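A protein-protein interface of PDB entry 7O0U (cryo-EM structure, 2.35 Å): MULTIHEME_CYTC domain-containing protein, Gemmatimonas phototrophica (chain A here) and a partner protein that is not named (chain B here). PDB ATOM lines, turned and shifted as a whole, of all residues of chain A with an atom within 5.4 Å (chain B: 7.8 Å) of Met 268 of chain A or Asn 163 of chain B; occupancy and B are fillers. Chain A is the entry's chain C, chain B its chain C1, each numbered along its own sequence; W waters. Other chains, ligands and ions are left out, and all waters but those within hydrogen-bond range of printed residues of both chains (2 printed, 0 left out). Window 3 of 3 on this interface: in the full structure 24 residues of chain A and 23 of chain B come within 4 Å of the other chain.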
ATOM      1  N   TYR A 162      33.423  19.933   1.309  1.00  0.00           N
ATOM      2  CA  TYR A 162      32.394  19.453   0.394  1.00  0.00           C
ATOM      3  C   TYR A 162      31.091  19.161   1.129  1.00  0.00           C
ATOM      4  O   TYR A 162      31.086  18.640   2.247  1.00  0.00           O
ATOM      5  CB  TYR A 162      32.854  18.186  -0.326  1.00  0.00           C
ATOM      6  CG  TYR A 162      34.026  18.359  -1.256  1.00  0.00           C
ATOM      7  CD1 TYR A 162      34.180  19.514  -2.008  1.00  0.00           C
ATOM      8  CD2 TYR A 162      34.967  17.351  -1.402  1.00  0.00           C
ATOM      9  CE1 TYR A 162      35.234  19.656  -2.885  1.00  0.00           C
ATOM     10  CE2 TYR A 162      36.035  17.492  -2.259  1.00  0.00           C
ATOM     11  CZ  TYR A 162      36.161  18.643  -3.003  1.00  0.00           C
ATOM     12  OH  TYR A 162      37.238  18.797  -3.843  1.00  0.00           O
ATOM     13  N   SER A 163      29.980  19.506   0.480  1.00  0.00           N
ATOM     14  CA  SER A 163      28.642  19.202   0.967  1.00  0.00           C
ATOM     15  C   SER A 163      27.715  18.941  -0.215  1.00  0.00           C
ATOM     16  O   SER A 163      27.827  17.904  -0.876  1.00  0.00           O
ATOM     17  CB  SER A 163      28.116  20.330   1.859  1.00  0.00           C
ATOM     18  OG  SER A 163      28.060  21.560   1.163  1.00  0.00           O
ATOM     19  N   SER A 164      26.801  19.869  -0.491  1.00  0.00           N
ATOM     20  CA  SER A 164      25.960  19.778  -1.677  1.00  0.00           C
ATOM     21  C   SER A 164      26.751  20.079  -2.951  1.00  0.00           C
ATOM     22  O   SER A 164      27.759  20.790  -2.934  1.00  0.00           O
ATOM     23  CB  SER A 164      24.777  20.737  -1.557  1.00  0.00           C
ATOM     24  OG  SER A 164      24.052  20.819  -2.770  1.00  0.00           O
ATOM     25  N   GLN A 165      26.273  19.519  -4.069  1.00  0.00           N
ATOM     26  CA  GLN A 165      26.766  19.905  -5.391  1.00  0.00           C
ATOM     27  C   GLN A 165      26.578  21.394  -5.673  1.00  0.00           C
ATOM     28  O   GLN A 165      27.462  22.039  -6.249  1.00  0.00           O
ATOM     29  CB  GLN A 165      26.056  19.086  -6.470  1.00  0.00           C
ATOM     30  CG  GLN A 165      26.354  17.600  -6.453  1.00  0.00           C
ATOM     31  CD  GLN A 165      25.571  16.844  -7.512  1.00  0.00           C
ATOM     32  OE1 GLN A 165      24.626  17.374  -8.096  1.00  0.00           O
ATOM     33  NE2 GLN A 165      25.964  15.602  -7.766  1.00  0.00           N
ATOM     34  N   GLY A 266      37.122  16.995   6.238  1.00  0.00           N
ATOM     35  CA  GLY A 266      35.681  17.035   6.120  1.00  0.00           C
ATOM     36  C   GLY A 266      35.033  15.662   6.155  1.00  0.00           C
ATOM     37  O   GLY A 266      35.697  14.627   6.183  1.00  0.00           O
ATOM     38  N   ALA A 267      33.697  15.670   6.158  1.00  0.00           N
ATOM     39  CA  ALA A 267      32.940  14.421   6.109  1.00  0.00           C
ATOM     40  C   ALA A 267      33.275  13.589   4.873  1.00  0.00           C
ATOM     41  O   ALA A 267      33.313  12.356   4.942  1.00  0.00           O
ATOM     42  CB  ALA A 267      31.442  14.720   6.161  1.00  0.00           C
ATOM     43  N   MET A 268      33.520  14.240   3.736  1.00  0.00           N
ATOM     44  CA  MET A 268      34.003  13.541   2.549  1.00  0.00           C
ATOM     45  C   MET A 268      35.493  13.229   2.599  1.00  0.00           C
ATOM     46  O   MET A 268      36.025  12.683   1.627  1.00  0.00           O
ATOM     47  CB  MET A 268      33.695  14.358   1.290  1.00  0.00           C
ATOM     48  CG  MET A 268      32.225  14.709   1.076  1.00  0.00           C
ATOM     49  SD  MET A 268      31.165  13.296   0.703  1.00  0.00           S
ATOM     50  CE  MET A 268      30.529  12.883   2.326  1.00  0.00           C
ATOM     51  N   GLY A 269      36.175  13.560   3.692  1.00  0.00           N
ATOM     52  CA  GLY A 269      37.611  13.397   3.782  1.00  0.00           C
ATOM     53  C   GLY A 269      38.417  14.424   3.024  1.00  0.00           C
ATOM     54  O   GLY A 269      39.622  14.226   2.832  1.00  0.00           O
ATOM     55  N   ASP A 270      37.792  15.507   2.577  1.00  0.00           N
ATOM     56  CA  ASP A 270      38.484  16.570   1.865  1.00  0.00           C
ATOM     57  C   ASP A 270      39.197  17.511   2.831  1.00  0.00           C
ATOM     58  O   ASP A 270      38.790  17.682   3.983  1.00  0.00           O
ATOM     59  CB  ASP A 270      37.504  17.345   0.987  1.00  0.00           C
ATOM     60  CG  ASP A 270      36.340  17.906   1.771  1.00  0.00           C
ATOM     61  OD1 ASP A 270      35.640  17.122   2.442  1.00  0.00           O
ATOM     62  OD2 ASP A 270      36.121  19.131   1.707  1.00  0.00           O
ATOM     63  N   GLN B 158      24.722  11.096  -9.870  1.00  0.00           N
ATOM     64  CA  GLN B 158      24.101  11.413  -8.588  1.00  0.00           C
ATOM     65  C   GLN B 158      25.124  11.429  -7.458  1.00  0.00           C
ATOM     66  O   GLN B 158      25.995  10.560  -7.372  1.00  0.00           O
ATOM     67  CB  GLN B 158      23.000  10.401  -8.268  1.00  0.00           C
ATOM     68  CG  GLN B 158      21.807  10.453  -9.201  1.00  0.00           C
ATOM     69  CD  GLN B 158      20.825   9.324  -8.951  1.00  0.00           C
ATOM     70  OE1 GLN B 158      20.796   8.740  -7.868  1.00  0.00           O
ATOM     71  NE2 GLN B 158      20.016   9.010  -9.956  1.00  0.00           N
ATOM     72  N   ALA B 159      25.008  12.426  -6.582  1.00  0.00           N
ATOM     73  CA  ALA B 159      25.720  12.414  -5.316  1.00  0.00           C
ATOM     74  C   ALA B 159      25.187  11.298  -4.418  1.00  0.00           C
ATOM     75  O   ALA B 159      24.060  10.832  -4.599  1.00  0.00           O
ATOM     76  CB  ALA B 159      25.577  13.766  -4.620  1.00  0.00           C
ATOM     77  N   PRO B 160      25.984  10.838  -3.449  1.00  0.00           N
ATOM     78  CA  PRO B 160      25.424   9.995  -2.385  1.00  0.00           C
ATOM     79  C   PRO B 160      24.243  10.693  -1.721  1.00  0.00           C
ATOM     80  O   PRO B 160      24.194  11.921  -1.637  1.00  0.00           O
ATOM     81  CB  PRO B 160      26.601   9.808  -1.418  1.00  0.00           C
ATOM     82  CG  PRO B 160      27.814  10.053  -2.252  1.00  0.00           C
ATOM     83  CD  PRO B 160      27.413  11.113  -3.232  1.00  0.00           C
ATOM     84  N   ILE B 161      23.284   9.893  -1.246  1.00  0.00           N
ATOM     85  CA  ILE B 161      22.043  10.457  -0.717  1.00  0.00           C
ATOM     86  C   ILE B 161      22.294  11.379   0.473  1.00  0.00           C
ATOM     87  O   ILE B 161      21.569  12.364   0.665  1.00  0.00           O
ATOM     88  CB  ILE B 161      21.051   9.328  -0.364  1.00  0.00           C
ATOM     89  CG1 ILE B 161      19.675   9.914  -0.042  1.00  0.00           C
ATOM     90  CG2 ILE B 161      21.566   8.479   0.789  1.00  0.00           C
ATOM     91  CD1 ILE B 161      18.545   8.921  -0.147  1.00  0.00           C
ATOM     92  N   THR B 162      23.320  11.097   1.280  1.00  0.00           N
ATOM     93  CA  THR B 162      23.689  11.978   2.385  1.00  0.00           C
ATOM     94  C   THR B 162      24.276  13.312   1.942  1.00  0.00           C
ATOM     95  O   THR B 162      24.504  14.174   2.796  1.00  0.00           O
ATOM     96  CB  THR B 162      24.688  11.274   3.304  1.00  0.00           C
ATOM     97  OG1 THR B 162      25.790  10.787   2.528  1.00  0.00           O
ATOM     98  CG2 THR B 162      24.027  10.114   4.023  1.00  0.00           C
ATOM     99  N   ASN B 163      24.528  13.510   0.650  1.00  0.00           N
ATOM    100  CA  ASN B 163      24.914  14.812   0.123  1.00  0.00           C
ATOM    101  C   ASN B 163      23.801  15.503  -0.656  1.00  0.00           C
ATOM    102  O   ASN B 163      24.054  16.525  -1.303  1.00  0.00           O
ATOM    103  CB  ASN B 163      26.164  14.666  -0.746  1.00  0.00           C
ATOM    104  CG  ASN B 163      27.392  14.309   0.067  1.00  0.00           C
ATOM    105  OD1 ASN B 163      27.878  15.113   0.860  1.00  0.00           O
ATOM    106  ND2 ASN B 163      27.889  13.092  -0.113  1.00  0.00           N
ATOM    107  N   GLN B 164      22.584  14.975  -0.619  1.00  0.00           N
ATOM    108  CA  GLN B 164      21.449  15.574  -1.308  1.00  0.00           C
ATOM    109  C   GLN B 164      20.638  16.414  -0.326  1.00  0.00           C
ATOM    110  O   GLN B 164      20.262  15.933   0.748  1.00  0.00           O
ATOM    111  CB  GLN B 164      20.593  14.482  -1.950  1.00  0.00           C
ATOM    112  CG  GLN B 164      21.368  13.683  -2.997  1.00  0.00           C
ATOM    113  CD  GLN B 164      20.534  12.625  -3.691  1.00  0.00           C
ATOM    114  OE1 GLN B 164      19.315  12.744  -3.790  1.00  0.00           O
ATOM    115  NE2 GLN B 164      21.194  11.579  -4.177  1.00  0.00           N
ATOM    116  N   ARG B 165      20.385  17.671  -0.692  1.00  0.00           N
ATOM    117  CA  ARG B 165      19.619  18.572   0.162  1.00  0.00           C
ATOM    118  C   ARG B 165      18.145  18.187   0.162  1.00  0.00           C
ATOM    119  O   ARG B 165      17.575  17.858  -0.881  1.00  0.00           O
ATOM    120  CB  ARG B 165      19.766  20.012  -0.331  1.00  0.00           C
ATOM    121  CG  ARG B 165      21.120  20.651  -0.082  1.00  0.00           C
ATOM    122  CD  ARG B 165      21.127  22.087  -0.585  1.00  0.00           C
ATOM    123  NE  ARG B 165      22.381  22.774  -0.303  1.00  0.00           N
ATOM    124  CZ  ARG B 165      22.687  23.986  -0.745  1.00  0.00           C
ATOM    125  NH1 ARG B 165      21.819  24.712  -1.430  1.00  0.00           N
ATOM    126  NH2 ARG B 165      23.887  24.490  -0.478  1.00  0.00           N
ATOM    127  N   ARG B 166      17.517  18.237   1.342  1.00  0.00           N
ATOM    128  CA  ARG B 166      16.060  18.143   1.391  1.00  0.00           C
ATOM    129  C   ARG B 166      15.373  19.408   0.890  1.00  0.00           C
ATOM    130  O   ARG B 166      14.274  19.329   0.332  1.00  0.00           O
ATOM    131  CB  ARG B 166      15.577  17.850   2.813  1.00  0.00           C
ATOM    132  CG  ARG B 166      15.984  16.515   3.403  1.00  0.00           C
ATOM    133  CD  ARG B 166      15.092  16.207   4.598  1.00  0.00           C
ATOM    134  NE  ARG B 166      15.677  15.249   5.525  1.00  0.00           N
ATOM    135  CZ  ARG B 166      15.084  14.135   5.932  1.00  0.00           C
ATOM    136  NH1 ARG B 166      14.051  13.627   5.282  1.00  0.00           N
ATOM    137  NH2 ARG B 166      15.590  13.472   6.966  1.00  0.00           N
ATOM    138  N   ARG B 189      19.013  19.009   7.230  1.00  0.00           N
ATOM    139  CA  ARG B 189      19.267  19.614   5.924  1.00  0.00           C
ATOM    140  C   ARG B 189      19.544  18.582   4.835  1.00  0.00           C
ATOM    141  O   ARG B 189      19.312  18.860   3.655  1.00  0.00           O
ATOM    142  CB  ARG B 189      20.440  20.587   6.027  1.00  0.00           C
ATOM    143  CG  ARG B 189      20.137  21.816   6.854  1.00  0.00           C
ATOM    144  CD  ARG B 189      21.374  22.661   7.077  1.00  0.00           C
ATOM    145  NE  ARG B 189      21.102  23.748   8.008  1.00  0.00           N
ATOM    146  CZ  ARG B 189      22.019  24.577   8.486  1.00  0.00           C
ATOM    147  NH1 ARG B 189      23.297  24.454   8.168  1.00  0.00           N
ATOM    148  NH2 ARG B 189      21.645  25.550   9.311  1.00  0.00           N
ATOM    149  N   TYR B 190      20.044  17.407   5.198  1.00  0.00           N
ATOM    150  CA  TYR B 190      20.390  16.377   4.230  1.00  0.00           C
ATOM    151  C   TYR B 190      19.602  15.107   4.517  1.00  0.00           C
ATOM    152  O   TYR B 190      19.225  14.837   5.660  1.00  0.00           O
ATOM    153  CB  TYR B 190      21.900  16.127   4.238  1.00  0.00           C
ATOM    154  CG  TYR B 190      22.648  17.334   3.727  1.00  0.00           C
ATOM    155  CD1 TYR B 190      22.832  17.535   2.367  1.00  0.00           C
ATOM    156  CD2 TYR B 190      23.106  18.310   4.600  1.00  0.00           C
ATOM    157  CE1 TYR B 190      23.508  18.639   1.895  1.00  0.00           C
ATOM    158  CE2 TYR B 190      23.766  19.430   4.136  1.00  0.00           C
ATOM    159  CZ  TYR B 190      23.967  19.587   2.783  1.00  0.00           C
ATOM    160  OH  TYR B 190      24.609  20.709   2.313  1.00  0.00           O
ATOM    161  N   TYR B 191      19.342  14.337   3.466  1.00  0.00           N
ATOM    162  CA  TYR B 191      18.722  13.034   3.646  1.00  0.00           C
ATOM    163  C   TYR B 191      19.619  12.113   4.470  1.00  0.00           C
ATOM    164  O   TYR B 191      20.847  12.147   4.331  1.00  0.00           O
ATOM    165  CB  TYR B 191      18.422  12.405   2.286  1.00  0.00           C
ATOM    166  CG  TYR B 191      17.278  13.077   1.570  1.00  0.00           C
ATOM    167  CD1 TYR B 191      15.964  12.740   1.857  1.00  0.00           C
ATOM    168  CD2 TYR B 191      17.509  14.074   0.633  1.00  0.00           C
ATOM    169  CE1 TYR B 191      14.914  13.363   1.222  1.00  0.00           C
ATOM    170  CE2 TYR B 191      16.464  14.702  -0.011  1.00  0.00           C
ATOM    171  CZ  TYR B 191      15.167  14.342   0.288  1.00  0.00           C
ATOM    172  OH  TYR B 191      14.119  14.956  -0.356  1.00  0.00           O
ATOM    173  N   PRO B 192      19.040  11.286   5.337  1.00  0.00           N
ATOM    174  CA  PRO B 192      19.844  10.343   6.117  1.00  0.00           C
ATOM    175  C   PRO B 192      20.344   9.191   5.260  1.00  0.00           C
ATOM    176  O   PRO B 192      19.847   8.931   4.162  1.00  0.00           O
ATOM    177  CB  PRO B 192      18.869   9.862   7.196  1.00  0.00           C
ATOM    178  CG  PRO B 192      17.540   9.934   6.532  1.00  0.00           C
ATOM    179  CD  PRO B 192      17.600  11.128   5.601  1.00  0.00           C
HETATM  180  O   HOH W   1      24.284  17.429  -3.863  1.00  0.00           O
HETATM  181  O   HOH W   2      26.123  23.478   1.037  1.00  0.00           O
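The side-chain amide nitrogen (NE2) of Gln 164 of chain B lies within hydrogen-bond range of the backbone carbonyl oxygen (O) of Ala 159 of chain B, 3.0 Å away.
The side-chain amide oxygen (OD1) of Asn 163 of chain B lies close to the backbone carbonyl oxygen (O) of Ser 163 of chain A.
The side-chain sulfur of Met 268 of chain A sits at hydrogen-bond distance from the side-chain amide nitrogen of Asn 163 of chain B, 3.4 Å away.
Printed residues of chain B within 4 Å of Ser 163 of chain A: Asn 163 (3.3 Å) and Tyr 190 (3.6 Å).
No residue of chain B comes within 4 Å of Ala 267 of chain A.
Met 268 of chain A touches just one residue of chain B: Asn 163.
Of the printed residues of chain A, Ala 159 of chain B touches Gln 165 (3.5 Å).
Of chain A, only Ser 163 (3.3 Å), Ser 164 (3.8 Å) and Met 268 (3.4 Å) come within 4 Å of Asn 163 of chain B.
Of the printed residues of chain A, Arg 165 of chain B touches Ser 164.
The nearest residue of chain A that does not touch Asn 163 of chain B is Gln 165 of chain A (4.6 Å).
The nearest printed residue of chain B that does not touch Ser 164 of chain A is Gln 164 of chain B (6.0 Å).
Among the printed residues, pairs that only touch across the chains: Ser 164 of chain A with Arg 165 of chain B (3.4 Å), Gln 165 of chain A with Ala 159 of chain B (3.5 Å), Ser 163 of chain A with Tyr 190 of chain B (3.6 Å), Ser 164 of chain A with Tyr 190 of chain B (3.7 Å) and Ser 164 of chain A with Asn 163 of chain B (3.8 Å).
Water W1 bridges O of Asn 163 of chain B and N of Gln 165 of chain A.
Water W2 lies within hydrogen-bond range of OG of Ser 163 of chain A (2.7 Å), NH2 of Arg 165 of chain B (2.9 Å) and OH of Tyr 190 of chain B (3.4 Å).
Hydrophobic or aromatic side chains of chain B within 4 Å of the printed part of chain A: Ala 159 and Tyr 190.
Among the printed residues, no Asp or Glu carboxylate lies within 4 Å of a Lys or Arg side-chain nitrogen of the other chain.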
